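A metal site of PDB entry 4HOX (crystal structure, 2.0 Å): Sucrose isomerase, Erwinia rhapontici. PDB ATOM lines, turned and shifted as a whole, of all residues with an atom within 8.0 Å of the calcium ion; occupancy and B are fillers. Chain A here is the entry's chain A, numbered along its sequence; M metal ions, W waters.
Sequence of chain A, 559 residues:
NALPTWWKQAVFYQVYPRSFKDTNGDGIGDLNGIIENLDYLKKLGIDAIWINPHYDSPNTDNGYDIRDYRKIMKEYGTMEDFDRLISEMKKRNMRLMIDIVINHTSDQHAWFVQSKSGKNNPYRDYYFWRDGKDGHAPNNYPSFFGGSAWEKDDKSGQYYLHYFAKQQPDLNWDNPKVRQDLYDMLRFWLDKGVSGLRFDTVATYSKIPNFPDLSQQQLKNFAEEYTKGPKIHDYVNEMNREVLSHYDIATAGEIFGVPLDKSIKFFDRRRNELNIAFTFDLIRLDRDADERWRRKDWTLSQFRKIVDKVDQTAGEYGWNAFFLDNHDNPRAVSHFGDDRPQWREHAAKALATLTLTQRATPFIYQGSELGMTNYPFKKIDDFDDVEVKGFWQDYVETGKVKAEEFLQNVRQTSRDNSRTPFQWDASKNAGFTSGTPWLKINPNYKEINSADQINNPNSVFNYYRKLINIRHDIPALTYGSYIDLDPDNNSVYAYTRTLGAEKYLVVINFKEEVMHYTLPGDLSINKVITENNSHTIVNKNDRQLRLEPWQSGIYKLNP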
ATOM      1  N   PRO A  17     -18.123  13.376  -3.238  1.00  0.00           N
ATOM      2  CA  PRO A  17     -17.867  12.785  -1.898  1.00  0.00           C
ATOM      3  C   PRO A  17     -16.596  13.315  -1.173  1.00  0.00           C
ATOM      4  O   PRO A  17     -16.607  13.494   0.046  1.00  0.00           O
ATOM      5  CB  PRO A  17     -17.733  11.264  -2.208  1.00  0.00           C
ATOM      6  CG  PRO A  17     -18.669  11.095  -3.395  1.00  0.00           C
ATOM      7  CD  PRO A  17     -18.381  12.319  -4.261  1.00  0.00           C
ATOM      8  N   ARG A  18     -15.579  13.644  -1.937  1.00  0.00           N
ATOM      9  CA  ARG A  18     -14.284  14.174  -1.418  1.00  0.00           C
ATOM     10  C   ARG A  18     -14.482  15.436  -0.547  1.00  0.00           C
ATOM     11  O   ARG A  18     -13.702  15.707   0.373  1.00  0.00           O
ATOM     12  CB  ARG A  18     -13.449  14.588  -2.642  1.00  0.00           C
ATOM     13  CG  ARG A  18     -11.995  14.768  -2.357  1.00  0.00           C
ATOM     14  CD  ARG A  18     -11.128  14.964  -3.583  1.00  0.00           C
ATOM     15  NE  ARG A  18      -9.803  15.221  -3.018  1.00  0.00           N
ATOM     16  CZ  ARG A  18      -8.909  14.273  -2.691  1.00  0.00           C
ATOM     17  NH1 ARG A  18      -9.094  12.990  -2.957  1.00  0.00           N
ATOM     18  NH2 ARG A  18      -7.761  14.647  -2.175  1.00  0.00           N
ATOM     19  N   LYS A  21     -18.609  15.502   3.443  1.00  0.00           N
ATOM     20  CA  LYS A  21     -18.448  15.419   4.912  1.00  0.00           C
ATOM     21  C   LYS A  21     -17.397  14.379   5.263  1.00  0.00           C
ATOM     22  O   LYS A  21     -17.541  13.228   4.897  1.00  0.00           O
ATOM     23  CB  LYS A  21     -19.764  15.043   5.597  1.00  0.00           C
ATOM     24  CG  LYS A  21     -19.655  14.838   7.110  1.00  0.00           C
ATOM     25  CD  LYS A  21     -19.564  16.144   7.881  1.00  0.00           C
ATOM     26  CE  LYS A  21     -19.252  15.920   9.370  1.00  0.00           C
ATOM     27  NZ  LYS A  21     -17.825  15.995   9.722  1.00  0.00           N
ATOM     28  N   ASP A  22     -16.350  14.810   6.014  1.00  0.00           N
ATOM     29  CA  ASP A  22     -15.281  13.901   6.488  1.00  0.00           C
ATOM     30  C   ASP A  22     -15.695  13.403   7.886  1.00  0.00           C
ATOM     31  O   ASP A  22     -16.048  14.233   8.767  1.00  0.00           O
ATOM     32  CB  ASP A  22     -13.964  14.661   6.581  1.00  0.00           C
ATOM     33  CG  ASP A  22     -12.852  13.845   7.247  1.00  0.00           C
ATOM     34  OD1 ASP A  22     -12.850  12.591   7.185  1.00  0.00           O
ATOM     35  OD2 ASP A  22     -11.947  14.497   7.805  1.00  0.00           O
ATOM     36  N   THR A  23     -15.703  12.093   8.092  1.00  0.00           N
ATOM     37  CA  THR A  23     -16.130  11.583   9.367  1.00  0.00           C
ATOM     38  C   THR A  23     -14.951  10.908  10.118  1.00  0.00           C
ATOM     39  O   THR A  23     -15.153  10.343  11.189  1.00  0.00           O
ATOM     40  CB  THR A  23     -17.315  10.586   9.211  1.00  0.00           C
ATOM     41  OG1 THR A  23     -16.877   9.503   8.403  1.00  0.00           O
ATOM     42  CG2 THR A  23     -18.589  11.293   8.552  1.00  0.00           C
ATOM     43  N   ASN A  24     -13.728  10.958   9.600  1.00  0.00           N
ATOM     44  CA  ASN A  24     -12.604  10.359  10.368  1.00  0.00           C
ATOM     45  C   ASN A  24     -11.345  11.223  10.476  1.00  0.00           C
ATOM     46  O   ASN A  24     -10.279  10.674  10.626  1.00  0.00           O
ATOM     47  CB  ASN A  24     -12.250   8.949   9.819  1.00  0.00           C
ATOM     48  CG  ASN A  24     -11.594   8.982   8.442  1.00  0.00           C
ATOM     49  OD1 ASN A  24     -11.611   9.979   7.723  1.00  0.00           O
ATOM     50  ND2 ASN A  24     -10.953   7.880   8.075  1.00  0.00           N
ATOM     51  N   GLY A  25     -11.494  12.544  10.325  1.00  0.00           N
ATOM     52  CA  GLY A  25     -10.422  13.528  10.506  1.00  0.00           C
ATOM     53  C   GLY A  25      -9.242  13.495   9.552  1.00  0.00           C
ATOM     54  O   GLY A  25      -8.238  14.129   9.815  1.00  0.00           O
ATOM     55  N   ASP A  26      -9.326  12.781   8.433  1.00  0.00           N
ATOM     56  CA  ASP A  26      -8.192  12.846   7.469  1.00  0.00           C
ATOM     57  C   ASP A  26      -8.317  14.049   6.489  1.00  0.00           C
ATOM     58  O   ASP A  26      -7.432  14.302   5.704  1.00  0.00           O
ATOM     59  CB  ASP A  26      -8.005  11.507   6.737  1.00  0.00           C
ATOM     60  CG  ASP A  26      -9.138  11.221   5.728  1.00  0.00           C
ATOM     61  OD1 ASP A  26     -10.249  11.839   5.787  1.00  0.00           O
ATOM     62  OD2 ASP A  26      -8.942  10.366   4.881  1.00  0.00           O
ATOM     63  N   GLY A  27      -9.407  14.818   6.585  1.00  0.00           N
ATOM     64  CA  GLY A  27      -9.599  16.028   5.797  1.00  0.00           C
ATOM     65  C   GLY A  27     -10.313  15.795   4.463  1.00  0.00           C
ATOM     66  O   GLY A  27     -10.474  16.707   3.689  1.00  0.00           O
ATOM     67  N   ILE A  28     -10.742  14.552   4.220  1.00  0.00           N
ATOM     68  CA  ILE A  28     -11.297  14.163   2.939  1.00  0.00           C
ATOM     69  C   ILE A  28     -12.669  13.605   3.244  1.00  0.00           C
ATOM     70  O   ILE A  28     -12.841  12.847   4.177  1.00  0.00           O
ATOM     71  CB  ILE A  28     -10.413  13.088   2.224  1.00  0.00           C
ATOM     72  CG1 ILE A  28      -9.054  13.710   1.863  1.00  0.00           C
ATOM     73  CG2 ILE A  28     -11.161  12.441   1.037  1.00  0.00           C
ATOM     74  CD1 ILE A  28      -7.993  12.685   1.453  1.00  0.00           C
ATOM     75  N   GLY A  29     -13.680  14.014   2.470  1.00  0.00           N
ATOM     76  CA  GLY A  29     -15.030  13.489   2.654  1.00  0.00           C
ATOM     77  C   GLY A  29     -15.092  11.991   2.362  1.00  0.00           C
ATOM     78  O   GLY A  29     -14.301  11.484   1.566  1.00  0.00           O
ATOM     79  N   ASP A  30     -16.045  11.302   2.958  1.00  0.00           N
ATOM     80  CA  ASP A  30     -16.119   9.843   2.793  1.00  0.00           C
ATOM     81  C   ASP A  30     -17.618   9.424   2.703  1.00  0.00           C
ATOM     82  O   ASP A  30     -18.512  10.253   2.917  1.00  0.00           O
ATOM     83  CB  ASP A  30     -15.340   9.204   3.964  1.00  0.00           C
ATOM     84  CG  ASP A  30     -15.693   9.865   5.287  1.00  0.00           C
ATOM     85  OD1 ASP A  30     -16.834   9.749   5.694  1.00  0.00           O
ATOM     86  OD2 ASP A  30     -14.857  10.539   5.928  1.00  0.00           O
ATOM     87  N   LEU A  31     -17.872   8.159   2.368  1.00  0.00           N
ATOM     88  CA  LEU A  31     -19.234   7.600   2.317  1.00  0.00           C
ATOM     89  C   LEU A  31     -19.975   7.706   3.598  1.00  0.00           C
ATOM     90  O   LEU A  31     -21.147   8.045   3.576  1.00  0.00           O
ATOM     91  CB  LEU A  31     -19.206   6.110   1.902  1.00  0.00           C
ATOM     92  CG  LEU A  31     -18.830   5.870   0.456  1.00  0.00           C
ATOM     93  CD1 LEU A  31     -18.524   4.356   0.302  1.00  0.00           C
ATOM     94  CD2 LEU A  31     -19.969   6.277  -0.534  1.00  0.00           C
ATOM     95  N   ASN A  32     -19.307   7.441   4.746  1.00  0.00           N
ATOM     96  CA  ASN A  32     -20.043   7.605   6.021  1.00  0.00           C
ATOM     97  C   ASN A  32     -20.582   9.044   6.222  1.00  0.00           C
ATOM     98  O   ASN A  32     -21.616   9.226   6.876  1.00  0.00           O
ATOM     99  CB  ASN A  32     -19.172   7.186   7.224  1.00  0.00           C
ATOM    100  CG  ASN A  32     -19.068   5.671   7.348  1.00  0.00           C
ATOM    101  OD1 ASN A  32     -19.902   4.930   6.817  1.00  0.00           O
ATOM    102  ND2 ASN A  32     -18.055   5.192   8.080  1.00  0.00           N
ATOM    103  N   GLY A  33     -19.857  10.041   5.722  1.00  0.00           N
ATOM    104  CA  GLY A  33     -20.325  11.422   5.836  1.00  0.00           C
ATOM    105  C   GLY A  33     -21.552  11.670   4.941  1.00  0.00           C
ATOM    106  O   GLY A  33     -22.413  12.478   5.295  1.00  0.00           O
ATOM    107  N   LYS A  74     -10.137   3.972  -1.350  1.00  0.00           N
ATOM    108  CA  LYS A  74      -9.683   3.814   0.047  1.00  0.00           C
ATOM    109  C   LYS A  74     -10.147   4.984   0.930  1.00  0.00           C
ATOM    110  O   LYS A  74     -10.609   4.799   2.037  1.00  0.00           O
ATOM    111  CB  LYS A  74      -8.156   3.731   0.049  1.00  0.00           C
ATOM    112  CG  LYS A  74      -7.509   3.176   1.321  1.00  0.00           C
ATOM    113  CD  LYS A  74      -5.997   3.486   1.288  1.00  0.00           C
ATOM    114  CE  LYS A  74      -5.150   2.670   2.261  1.00  0.00           C
ATOM    115  NZ  LYS A  74      -5.854   2.298   3.532  1.00  0.00           N
ATOM    116  N   GLU A  75     -10.019   6.198   0.437  1.00  0.00           N
ATOM    117  CA  GLU A  75     -10.421   7.389   1.189  1.00  0.00           C
ATOM    118  C   GLU A  75     -11.917   7.436   1.501  1.00  0.00           C
ATOM    119  O   GLU A  75     -12.333   8.071   2.483  1.00  0.00           O
ATOM    120  CB  GLU A  75     -10.022   8.652   0.394  1.00  0.00           C
ATOM    121  CG  GLU A  75      -8.523   8.955   0.309  1.00  0.00           C
ATOM    122  CD  GLU A  75      -7.764   8.174  -0.797  1.00  0.00           C
ATOM    123  OE1 GLU A  75      -8.336   7.399  -1.627  1.00  0.00           O
ATOM    124  OE2 GLU A  75      -6.534   8.361  -0.871  1.00  0.00           O
ATOM    125  N   TYR A  76     -12.744   6.790   0.687  1.00  0.00           N
ATOM    126  CA  TYR A  76     -14.198   6.923   0.952  1.00  0.00           C
ATOM    127  C   TYR A  76     -14.781   5.871   1.900  1.00  0.00           C
ATOM    128  O   TYR A  76     -15.916   6.004   2.371  1.00  0.00           O
ATOM    129  CB  TYR A  76     -14.986   6.974  -0.371  1.00  0.00           C
ATOM    130  CG  TYR A  76     -14.643   8.161  -1.297  1.00  0.00           C
ATOM    131  CD1 TYR A  76     -13.888   9.274  -0.838  1.00  0.00           C
ATOM    132  CD2 TYR A  76     -15.020   8.135  -2.638  1.00  0.00           C
ATOM    133  CE1 TYR A  76     -13.578  10.349  -1.675  1.00  0.00           C
ATOM    134  CE2 TYR A  76     -14.741   9.198  -3.484  1.00  0.00           C
ATOM    135  CZ  TYR A  76     -14.022  10.294  -3.012  1.00  0.00           C
ATOM    136  OH  TYR A  76     -13.734  11.280  -3.897  1.00  0.00           O
ATOM    137  N   GLY A  77     -14.059   4.740   2.059  1.00  0.00           N
ATOM    138  CA  GLY A  77     -14.510   3.661   2.994  1.00  0.00           C
ATOM    139  C   GLY A  77     -14.424   2.287   2.371  1.00  0.00           C
ATOM    140  O   GLY A  77     -13.549   2.041   1.623  1.00  0.00           O
ATOM    141  N   PHE A 432     -16.886  20.639   8.660  1.00  0.00           N
ATOM    142  CA  PHE A 432     -16.631  19.650   7.614  1.00  0.00           C
ATOM    143  C   PHE A 432     -15.737  18.448   8.096  1.00  0.00           C
ATOM    144  O   PHE A 432     -15.894  17.321   7.628  1.00  0.00           O
ATOM    145  CB  PHE A 432     -15.945  20.309   6.403  1.00  0.00           C
ATOM    146  CG  PHE A 432     -15.355  19.304   5.439  1.00  0.00           C
ATOM    147  CD1 PHE A 432     -16.199  18.511   4.629  1.00  0.00           C
ATOM    148  CD2 PHE A 432     -13.974  19.195   5.287  1.00  0.00           C
ATOM    149  CE1 PHE A 432     -15.649  17.568   3.774  1.00  0.00           C
ATOM    150  CE2 PHE A 432     -13.427  18.246   4.408  1.00  0.00           C
ATOM    151  CZ  PHE A 432     -14.270  17.423   3.648  1.00  0.00           C
ATOM    152  N   THR A 433     -14.800  18.735   8.993  1.00  0.00           N
ATOM    153  CA  THR A 433     -13.750  17.792   9.372  1.00  0.00           C
ATOM    154  C   THR A 433     -13.244  18.170  10.754  1.00  0.00           C
ATOM    155  O   THR A 433     -13.238  19.327  11.098  1.00  0.00           O
ATOM    156  CB  THR A 433     -12.557  17.778   8.377  1.00  0.00           C
ATOM    157  OG1 THR A 433     -11.603  16.790   8.783  1.00  0.00           O
ATOM    158  CG2 THR A 433     -11.849  19.126   8.264  1.00  0.00           C
HETATM  159 CA    CA M   1     -12.504  10.908   5.654  1.00  0.00          CA
HETATM  160  O   HOH W   1     -12.566   8.406   5.505  1.00  0.00           O
HETATM  161  O   HOH W   2     -11.507  10.110   3.647  1.00  0.00           O
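The side-chain carboxylate (OD2) of Asp 22 lies within hydrogen-bond range of the backbone NH (N) of Gly 25. The backbone NH (N) of Gly 27 lies within hydrogen-bond range of the side-chain carboxylate (OD2) of Asp 22 (2.8 Å). The side-chain hydroxyl (OG1) of Thr 433 lies within hydrogen-bond range of the side-chain carboxylate (OD2) of Asp 22. N of Asp 22 sits at hydrogen-bond distance from O of Phe 432 (3.0 Å). The side-chain carboxylate (OD1) of Asp 30 sits at hydrogen-bond distance from the side-chain hydroxyl (OG1) of Thr 23, at 2.7 Å. O of Lys 21 is in hydrogen-bond range of N of Asp 30, at 3.1 Å. The side-chain carboxylate of Asp 30 is in hydrogen-bond range of the backbone NH of Gly 33.
Five residues have an atom within 4 Å of the calcium ion: Asp 22, Asn 24, Asp 26, Ile 28 and Asp 30.
The calcium ion is bound by OD1 of Asp 22 (2.3 Å), water W2 (2.4 Å), OD2 of Asp 30 (2.4 Å), OD1 of Asn 24 (2.4 Å), OD1 of Asp 26 (2.4 Å), O of Ile 28 (2.5 Å) and water W1 (2.5 Å). The calcium ion has seven donor atoms within binding distance.
Water W1 lies within hydrogen-bond range of the backbone carbonyl oxygen of Glu 75 and the side-chain amide nitrogen of Asn 24. Water W2 bridges the backbone carbonyl oxygen of Glu 75 (2.5 Å) and the side-chain carboxylate of Asp 26 (2.9 Å).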
